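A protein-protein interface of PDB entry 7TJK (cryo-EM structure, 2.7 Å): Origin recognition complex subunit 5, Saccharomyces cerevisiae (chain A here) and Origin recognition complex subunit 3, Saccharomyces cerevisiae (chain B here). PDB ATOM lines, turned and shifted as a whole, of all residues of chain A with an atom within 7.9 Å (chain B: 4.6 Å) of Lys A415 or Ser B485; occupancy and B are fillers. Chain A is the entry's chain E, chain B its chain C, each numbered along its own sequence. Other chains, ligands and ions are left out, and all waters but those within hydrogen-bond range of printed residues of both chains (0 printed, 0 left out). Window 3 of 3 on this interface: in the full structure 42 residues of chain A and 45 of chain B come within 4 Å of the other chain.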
ATOM      1  N   ILE A 327      -6.468 -15.958  13.763  1.00  0.00           N
ATOM      2  CA  ILE A 327      -5.285 -15.524  14.496  1.00  0.00           C
ATOM      3  C   ILE A 327      -4.070 -15.509  13.578  1.00  0.00           C
ATOM      4  O   ILE A 327      -3.277 -14.562  13.601  1.00  0.00           O
ATOM      5  CB  ILE A 327      -5.079 -16.429  15.728  1.00  0.00           C
ATOM      6  CG1 ILE A 327      -6.174 -16.162  16.764  1.00  0.00           C
ATOM      7  CG2 ILE A 327      -3.699 -16.230  16.355  1.00  0.00           C
ATOM      8  CD1 ILE A 327      -6.053 -16.996  18.020  1.00  0.00           C
ATOM      9  N   LEU A 387       3.235  -8.624  18.563  1.00  0.00           N
ATOM     10  CA  LEU A 387       2.087  -8.930  19.408  1.00  0.00           C
ATOM     11  C   LEU A 387       1.301  -7.674  19.778  1.00  0.00           C
ATOM     12  O   LEU A 387       0.069  -7.724  19.879  1.00  0.00           O
ATOM     13  CB  LEU A 387       2.554  -9.674  20.656  1.00  0.00           C
ATOM     14  CG  LEU A 387       3.237 -11.016  20.399  1.00  0.00           C
ATOM     15  CD1 LEU A 387       3.825 -11.554  21.685  1.00  0.00           C
ATOM     16  CD2 LEU A 387       2.266 -12.011  19.786  1.00  0.00           C
ATOM     17  N   PHE A 390      -0.623  -6.798  16.688  1.00  0.00           N
ATOM     18  CA  PHE A 390      -1.627  -7.851  16.552  1.00  0.00           C
ATOM     19  C   PHE A 390      -2.823  -7.621  17.467  1.00  0.00           C
ATOM     20  O   PHE A 390      -3.970  -7.758  17.032  1.00  0.00           O
ATOM     21  CB  PHE A 390      -0.986  -9.215  16.840  1.00  0.00           C
ATOM     22  CG  PHE A 390      -1.969 -10.355  16.922  1.00  0.00           C
ATOM     23  CD1 PHE A 390      -2.472 -10.934  15.769  1.00  0.00           C
ATOM     24  CD2 PHE A 390      -2.363 -10.871  18.152  1.00  0.00           C
ATOM     25  CE1 PHE A 390      -3.368 -11.987  15.838  1.00  0.00           C
ATOM     26  CE2 PHE A 390      -3.260 -11.918  18.228  1.00  0.00           C
ATOM     27  CZ  PHE A 390      -3.762 -12.480  17.068  1.00  0.00           C
ATOM     28  N   GLN A 391      -2.588  -7.266  18.730  1.00  0.00           N
ATOM     29  CA  GLN A 391      -3.733  -6.963  19.578  1.00  0.00           C
ATOM     30  C   GLN A 391      -4.282  -5.562  19.343  1.00  0.00           C
ATOM     31  O   GLN A 391      -5.392  -5.268  19.801  1.00  0.00           O
ATOM     32  CB  GLN A 391      -3.398  -7.121  21.061  1.00  0.00           C
ATOM     33  CG  GLN A 391      -2.385  -6.136  21.577  1.00  0.00           C
ATOM     34  CD  GLN A 391      -2.228  -6.217  23.076  1.00  0.00           C
ATOM     35  OE1 GLN A 391      -1.377  -5.550  23.659  1.00  0.00           O
ATOM     36  NE2 GLN A 391      -3.034  -7.052  23.707  1.00  0.00           N
ATOM     37  N   PHE A 394      -6.682  -6.654  16.279  1.00  0.00           N
ATOM     38  CA  PHE A 394      -7.542  -7.825  16.361  1.00  0.00           C
ATOM     39  C   PHE A 394      -8.967  -7.419  16.728  1.00  0.00           C
ATOM     40  O   PHE A 394      -9.168  -6.441  17.456  1.00  0.00           O
ATOM     41  CB  PHE A 394      -7.020  -8.835  17.391  1.00  0.00           C
ATOM     42  CG  PHE A 394      -7.511 -10.237  17.169  1.00  0.00           C
ATOM     43  CD1 PHE A 394      -7.091 -10.960  16.062  1.00  0.00           C
ATOM     44  CD2 PHE A 394      -8.377 -10.837  18.069  1.00  0.00           C
ATOM     45  CE1 PHE A 394      -7.536 -12.251  15.848  1.00  0.00           C
ATOM     46  CE2 PHE A 394      -8.822 -12.129  17.866  1.00  0.00           C
ATOM     47  CZ  PHE A 394      -8.401 -12.838  16.752  1.00  0.00           C
ATOM     48  N   GLU A 410     -14.544  -8.998  31.650  1.00  0.00           N
ATOM     49  CA  GLU A 410     -14.599  -9.499  30.283  1.00  0.00           C
ATOM     50  C   GLU A 410     -13.283  -9.375  29.523  1.00  0.00           C
ATOM     51  O   GLU A 410     -13.034 -10.198  28.633  1.00  0.00           O
ATOM     52  CB  GLU A 410     -15.731  -8.797  29.518  1.00  0.00           C
ATOM     53  CG  GLU A 410     -15.663  -7.275  29.488  1.00  0.00           C
ATOM     54  CD  GLU A 410     -14.878  -6.739  28.314  1.00  0.00           C
ATOM     55  OE1 GLU A 410     -14.704  -7.482  27.325  1.00  0.00           O
ATOM     56  OE2 GLU A 410     -14.437  -5.573  28.379  1.00  0.00           O
ATOM     57  N   GLU A 411     -12.447  -8.380  29.858  1.00  0.00           N
ATOM     58  CA  GLU A 411     -11.071  -8.225  29.360  1.00  0.00           C
ATOM     59  C   GLU A 411     -11.031  -8.104  27.830  1.00  0.00           C
ATOM     60  O   GLU A 411     -10.618  -9.023  27.118  1.00  0.00           O
ATOM     61  CB  GLU A 411     -10.169  -9.363  29.856  1.00  0.00           C
ATOM     62  CG  GLU A 411      -9.824  -9.278  31.335  1.00  0.00           C
ATOM     63  CD  GLU A 411      -8.946  -8.084  31.666  1.00  0.00           C
ATOM     64  OE1 GLU A 411      -8.089  -7.723  30.833  1.00  0.00           O
ATOM     65  OE2 GLU A 411      -9.114  -7.508  32.761  1.00  0.00           O
ATOM     66  N   SER A 412     -11.523  -6.949  27.360  1.00  0.00           N
ATOM     67  CA  SER A 412     -11.756  -6.611  25.954  1.00  0.00           C
ATOM     68  C   SER A 412     -10.605  -6.916  24.998  1.00  0.00           C
ATOM     69  O   SER A 412     -10.839  -7.379  23.877  1.00  0.00           O
ATOM     70  CB  SER A 412     -12.086  -5.119  25.827  1.00  0.00           C
ATOM     71  OG  SER A 412     -13.251  -4.772  26.550  1.00  0.00           O
ATOM     72  N   LEU A 413      -9.370  -6.665  25.419  1.00  0.00           N
ATOM     73  CA  LEU A 413      -8.227  -6.837  24.532  1.00  0.00           C
ATOM     74  C   LEU A 413      -7.856  -8.317  24.431  1.00  0.00           C
ATOM     75  O   LEU A 413      -8.409  -9.176  25.124  1.00  0.00           O
ATOM     76  CB  LEU A 413      -7.056  -5.983  25.006  1.00  0.00           C
ATOM     77  CG  LEU A 413      -6.896  -4.642  24.282  1.00  0.00           C
ATOM     78  CD1 LEU A 413      -5.579  -4.004  24.644  1.00  0.00           C
ATOM     79  CD2 LEU A 413      -7.006  -4.804  22.768  1.00  0.00           C
ATOM     80  N   MET A 414      -6.902  -8.625  23.558  1.00  0.00           N
ATOM     81  CA  MET A 414      -6.498  -9.994  23.271  1.00  0.00           C
ATOM     82  C   MET A 414      -5.192 -10.297  23.987  1.00  0.00           C
ATOM     83  O   MET A 414      -4.212  -9.561  23.838  1.00  0.00           O
ATOM     84  CB  MET A 414      -6.336 -10.211  21.765  1.00  0.00           C
ATOM     85  CG  MET A 414      -5.832 -11.588  21.381  1.00  0.00           C
ATOM     86  SD  MET A 414      -7.138 -12.829  21.449  1.00  0.00           S
ATOM     87  CE  MET A 414      -6.383 -14.164  20.530  1.00  0.00           C
ATOM     88  N   LYS A 415      -5.179 -11.377  24.758  1.00  0.00           N
ATOM     89  CA  LYS A 415      -3.978 -11.835  25.437  1.00  0.00           C
ATOM     90  C   LYS A 415      -3.136 -12.687  24.496  1.00  0.00           C
ATOM     91  O   LYS A 415      -3.655 -13.343  23.590  1.00  0.00           O
ATOM     92  CB  LYS A 415      -4.330 -12.637  26.692  1.00  0.00           C
ATOM     93  CG  LYS A 415      -5.271 -11.923  27.646  1.00  0.00           C
ATOM     94  CD  LYS A 415      -5.423 -12.698  28.944  1.00  0.00           C
ATOM     95  CE  LYS A 415      -5.657 -11.767  30.121  1.00  0.00           C
ATOM     96  NZ  LYS A 415      -6.027 -12.516  31.353  1.00  0.00           N
ATOM     97  N   ALA A 416      -1.822 -12.665  24.719  1.00  0.00           N
ATOM     98  CA  ALA A 416      -0.887 -13.478  23.943  1.00  0.00           C
ATOM     99  C   ALA A 416      -0.733 -14.832  24.631  1.00  0.00           C
ATOM    100  O   ALA A 416       0.288 -15.146  25.246  1.00  0.00           O
ATOM    101  CB  ALA A 416       0.451 -12.766  23.793  1.00  0.00           C
ATOM    102  N   ASN A 417      -1.776 -15.648  24.515  1.00  0.00           N
ATOM    103  CA  ASN A 417      -1.785 -16.973  25.111  1.00  0.00           C
ATOM    104  C   ASN A 417      -1.074 -17.960  24.183  1.00  0.00           C
ATOM    105  O   ASN A 417      -0.457 -17.572  23.187  1.00  0.00           O
ATOM    106  CB  ASN A 417      -3.218 -17.384  25.445  1.00  0.00           C
ATOM    107  CG  ASN A 417      -4.060 -17.634  24.219  1.00  0.00           C
ATOM    108  OD1 ASN A 417      -3.853 -17.029  23.168  1.00  0.00           O
ATOM    109  ND2 ASN A 417      -5.035 -18.523  24.355  1.00  0.00           N
ATOM    110  N   ILE A 418      -1.160 -19.258  24.495  1.00  0.00           N
ATOM    111  CA  ILE A 418      -0.324 -20.254  23.825  1.00  0.00           C
ATOM    112  C   ILE A 418      -0.741 -20.538  22.390  1.00  0.00           C
ATOM    113  O   ILE A 418       0.085 -21.020  21.605  1.00  0.00           O
ATOM    114  CB  ILE A 418      -0.295 -21.581  24.612  1.00  0.00           C
ATOM    115  CG1 ILE A 418      -1.677 -22.228  24.644  1.00  0.00           C
ATOM    116  CG2 ILE A 418       0.206 -21.353  26.026  1.00  0.00           C
ATOM    117  CD1 ILE A 418      -1.629 -23.718  24.718  1.00  0.00           C
ATOM    118  N   GLU A 419      -1.979 -20.233  22.008  1.00  0.00           N
ATOM    119  CA  GLU A 419      -2.427 -20.509  20.650  1.00  0.00           C
ATOM    120  C   GLU A 419      -2.001 -19.441  19.654  1.00  0.00           C
ATOM    121  O   GLU A 419      -1.796 -19.758  18.478  1.00  0.00           O
ATOM    122  CB  GLU A 419      -3.949 -20.685  20.621  1.00  0.00           C
ATOM    123  CG  GLU A 419      -4.729 -19.521  21.186  1.00  0.00           C
ATOM    124  CD  GLU A 419      -6.220 -19.750  21.152  1.00  0.00           C
ATOM    125  OE1 GLU A 419      -6.640 -20.915  20.982  1.00  0.00           O
ATOM    126  OE2 GLU A 419      -6.977 -18.767  21.296  1.00  0.00           O
ATOM    127  N   VAL A 420      -1.818 -18.198  20.110  1.00  0.00           N
ATOM    128  CA  VAL A 420      -1.208 -17.166  19.277  1.00  0.00           C
ATOM    129  C   VAL A 420       0.235 -17.532  18.946  1.00  0.00           C
ATOM    130  O   VAL A 420       0.669 -17.433  17.791  1.00  0.00           O
ATOM    131  CB  VAL A 420      -1.310 -15.799  19.980  1.00  0.00           C
ATOM    132  CG1 VAL A 420      -0.557 -14.724  19.209  1.00  0.00           C
ATOM    133  CG2 VAL A 420      -2.766 -15.403  20.162  1.00  0.00           C
ATOM    134  N   PHE A 421       0.987 -18.002  19.945  1.00  0.00           N
ATOM    135  CA  PHE A 421       2.363 -18.428  19.709  1.00  0.00           C
ATOM    136  C   PHE A 421       2.428 -19.711  18.888  1.00  0.00           C
ATOM    137  O   PHE A 421       3.358 -19.882  18.091  1.00  0.00           O
ATOM    138  CB  PHE A 421       3.090 -18.611  21.038  1.00  0.00           C
ATOM    139  CG  PHE A 421       3.442 -17.324  21.713  1.00  0.00           C
ATOM    140  CD1 PHE A 421       4.632 -16.676  21.422  1.00  0.00           C
ATOM    141  CD2 PHE A 421       2.585 -16.759  22.641  1.00  0.00           C
ATOM    142  CE1 PHE A 421       4.957 -15.486  22.046  1.00  0.00           C
ATOM    143  CE2 PHE A 421       2.904 -15.571  23.269  1.00  0.00           C
ATOM    144  CZ  PHE A 421       4.092 -14.935  22.971  1.00  0.00           C
ATOM    145  N   SER B 482      -3.217 -18.574  29.416  1.00  0.00           N
ATOM    146  CA  SER B 482      -2.598 -17.287  29.105  1.00  0.00           C
ATOM    147  C   SER B 482      -1.246 -17.264  29.801  1.00  0.00           C
ATOM    148  O   SER B 482      -1.073 -16.617  30.831  1.00  0.00           O
ATOM    149  CB  SER B 482      -3.482 -16.129  29.547  1.00  0.00           C
ATOM    150  OG  SER B 482      -3.504 -16.014  30.959  1.00  0.00           O
ATOM    151  N   TYR B 483      -0.286 -17.973  29.197  1.00  0.00           N
ATOM    152  CA  TYR B 483       1.007 -18.317  29.790  1.00  0.00           C
ATOM    153  C   TYR B 483       1.816 -17.081  30.178  1.00  0.00           C
ATOM    154  O   TYR B 483       2.221 -16.927  31.338  1.00  0.00           O
ATOM    155  CB  TYR B 483       1.764 -19.198  28.780  1.00  0.00           C
ATOM    156  CG  TYR B 483       3.212 -19.551  29.067  1.00  0.00           C
ATOM    157  CD1 TYR B 483       4.255 -18.714  28.670  1.00  0.00           C
ATOM    158  CD2 TYR B 483       3.540 -20.754  29.675  1.00  0.00           C
ATOM    159  CE1 TYR B 483       5.569 -19.042  28.917  1.00  0.00           C
ATOM    160  CE2 TYR B 483       4.857 -21.093  29.914  1.00  0.00           C
ATOM    161  CZ  TYR B 483       5.865 -20.233  29.538  1.00  0.00           C
ATOM    162  OH  TYR B 483       7.178 -20.563  29.777  1.00  0.00           O
ATOM    163  N   LYS B 484       2.041 -16.191  29.209  1.00  0.00           N
ATOM    164  CA  LYS B 484       2.783 -14.956  29.437  1.00  0.00           C
ATOM    165  C   LYS B 484       2.048 -14.055  30.422  1.00  0.00           C
ATOM    166  O   LYS B 484       2.649 -13.482  31.338  1.00  0.00           O
ATOM    167  CB  LYS B 484       3.004 -14.249  28.097  1.00  0.00           C
ATOM    168  CG  LYS B 484       3.727 -12.920  28.170  1.00  0.00           C
ATOM    169  CD  LYS B 484       4.011 -12.396  26.769  1.00  0.00           C
ATOM    170  CE  LYS B 484       4.766 -11.078  26.805  1.00  0.00           C
ATOM    171  NZ  LYS B 484       3.922  -9.968  27.327  1.00  0.00           N
ATOM    172  N   SER B 485       0.725 -13.963  30.263  1.00  0.00           N
ATOM    173  CA  SER B 485      -0.090 -13.175  31.180  1.00  0.00           C
ATOM    174  C   SER B 485      -0.116 -13.785  32.574  1.00  0.00           C
ATOM    175  O   SER B 485      -0.169 -13.056  33.568  1.00  0.00           O
ATOM    176  CB  SER B 485      -1.509 -13.034  30.630  1.00  0.00           C
ATOM    177  OG  SER B 485      -2.354 -12.390  31.568  1.00  0.00           O
ATOM    178  N   ASN B 486      -0.072 -15.120  32.668  1.00  0.00           N
ATOM    179  CA  ASN B 486       0.000 -15.770  33.976  1.00  0.00           C
ATOM    180  C   ASN B 486       1.306 -15.447  34.684  1.00  0.00           C
ATOM    181  O   ASN B 486       1.306 -15.171  35.890  1.00  0.00           O
ATOM    182  CB  ASN B 486      -0.163 -17.282  33.838  1.00  0.00           C
ATOM    183  CG  ASN B 486      -1.612 -17.705  33.788  1.00  0.00           C
ATOM    184  OD1 ASN B 486      -2.450 -17.159  34.502  1.00  0.00           O
ATOM    185  ND2 ASN B 486      -1.917 -18.680  32.939  1.00  0.00           N
ATOM    186  N   ILE B 487       2.420 -15.449  33.940  1.00  0.00           N
ATOM    187  CA  ILE B 487       3.713 -15.058  34.508  1.00  0.00           C
ATOM    188  C   ILE B 487       3.679 -13.604  34.974  1.00  0.00           C
ATOM    189  O   ILE B 487       4.157 -13.275  36.069  1.00  0.00           O
ATOM    190  CB  ILE B 487       4.838 -15.298  33.483  1.00  0.00           C
ATOM    191  CG1 ILE B 487       4.951 -16.784  33.145  1.00  0.00           C
ATOM    192  CG2 ILE B 487       6.174 -14.795  34.007  1.00  0.00           C
ATOM    193  CD1 ILE B 487       5.197 -17.659  34.338  1.00  0.00           C
ATOM    194  N   GLU B 488       3.076 -12.724  34.169  1.00  0.00           N
ATOM    195  CA  GLU B 488       3.013 -11.303  34.512  1.00  0.00           C
ATOM    196  C   GLU B 488       2.134 -11.038  35.736  1.00  0.00           C
ATOM    197  O   GLU B 488       2.506 -10.241  36.605  1.00  0.00           O
ATOM    198  CB  GLU B 488       2.520 -10.510  33.306  1.00  0.00           C
ATOM    199  CG  GLU B 488       3.520 -10.479  32.164  1.00  0.00           C
ATOM    200  CD  GLU B 488       2.876 -10.141  30.837  1.00  0.00           C
ATOM    201  OE1 GLU B 488       1.628 -10.102  30.773  1.00  0.00           O
ATOM    202  OE2 GLU B 488       3.612  -9.918  29.856  1.00  0.00           O
ATOM    203  N   ASP B 489       0.973 -11.698  35.830  1.00  0.00           N
ATOM    204  CA  ASP B 489       0.119 -11.495  37.000  1.00  0.00           C
ATOM    205  C   ASP B 489       0.675 -12.175  38.244  1.00  0.00           C
ATOM    206  O   ASP B 489       0.360 -11.752  39.362  1.00  0.00           O
ATOM    207  CB  ASP B 489      -1.313 -11.975  36.745  1.00  0.00           C
ATOM    208  CG  ASP B 489      -1.947 -11.336  35.525  1.00  0.00           C
ATOM    209  OD1 ASP B 489      -1.894 -10.096  35.411  1.00  0.00           O
ATOM    210  OD2 ASP B 489      -2.560 -12.062  34.716  1.00  0.00           O
ATOM    211  N   ILE B 616      -0.218  -7.770  27.040  1.00  0.00           N
ATOM    212  CA  ILE B 616      -0.216  -8.124  25.629  1.00  0.00           C
ATOM    213  C   ILE B 616      -0.501  -9.613  25.457  1.00  0.00           C
ATOM    214  O   ILE B 616      -1.267 -10.011  24.578  1.00  0.00           O
ATOM    215  CB  ILE B 616       1.112  -7.731  24.959  1.00  0.00           C
ATOM    216  CG1 ILE B 616       1.496  -6.300  25.346  1.00  0.00           C
ATOM    217  CG2 ILE B 616       1.012  -7.886  23.456  1.00  0.00           C
ATOM    218  CD1 ILE B 616       2.674  -5.744  24.578  1.00  0.00           C
ATOM    219  OXT ILE B 616       0.010 -10.452  26.199  1.00  0.00           O
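The chain-end carboxylate of Ile B616 sits at hydrogen-bond distance from the backbone NH of Ala A416 (2.7 Å).
The backbone carbonyl oxygen of Met A414 sits close to the chain-end carboxylate of Ile B616 (3.1 Å).
The backbone carbonyl oxygen (O) of Ser B482 sits at hydrogen-bond distance from the side-chain amide nitrogen (ND2) of Asn B486, at 3.1 Å.
NE2 of Gln A391 lies within hydrogen-bond range of O of Met A414 (2.8 Å).
OD2 of Asp B489 lies within hydrogen-bond range of OG of Ser B485 (3.2 Å).
Leu A387 touches Ile B616.
Gln A391 touches Ile B616.
CB of Ser B482 touches CD of Lys A415, at 3.99 Å.
CE of Lys A415 touches OG of Ser B485, at 3.7 Å.
Ile B616 touches Lys A415 (O to C, 3.3 Å).
Ser B482 touches Asn A417 (CA to CB, 3.7 Å).
Ile A418 touches Tyr B483 (CG2 to CB, 3.8 Å).
Printed residues of chain B within 4 Å of Lys A415: Ser B482, Ser B485 and Ile B616.
Of the printed residues of chain A, Ile B616 touches Leu A387 (3.7 Å), Gln A391 (3.3 Å), Met A414 (3.1 Å), Lys A415 (3.3 Å) and Ala A416 (2.7 Å).
Printed residues of chain B within 4 Å of Gln A391: Ile B616.
Printed residues of chain B within 4 Å of Ile A418: Tyr B483.
Of the printed residues of chain A, Ser B482 touches Lys A415 and Asn A417.
Of the printed residues of chain B, Met A414 touches Ile B616.
Ile B487 touches none of the printed residues of chain A.
Phe A421 touches none of the printed residues of chain B.
The nearest residue of chain A that does not touch Ser B485 is Ala A416 (5.2 Å).
The nearest printed residue of chain B that does not touch Ile A418 is Ser B482 (5.2 Å).
Hydrophobic or aromatic side chains of chain A that line the printed part of chain B: Leu A387, Ala A416 and Ile A418.
Among the printed residues, no Asp or Glu carboxylate lies within 4 Å of a Lys or Arg side-chain nitrogen of the other chain.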
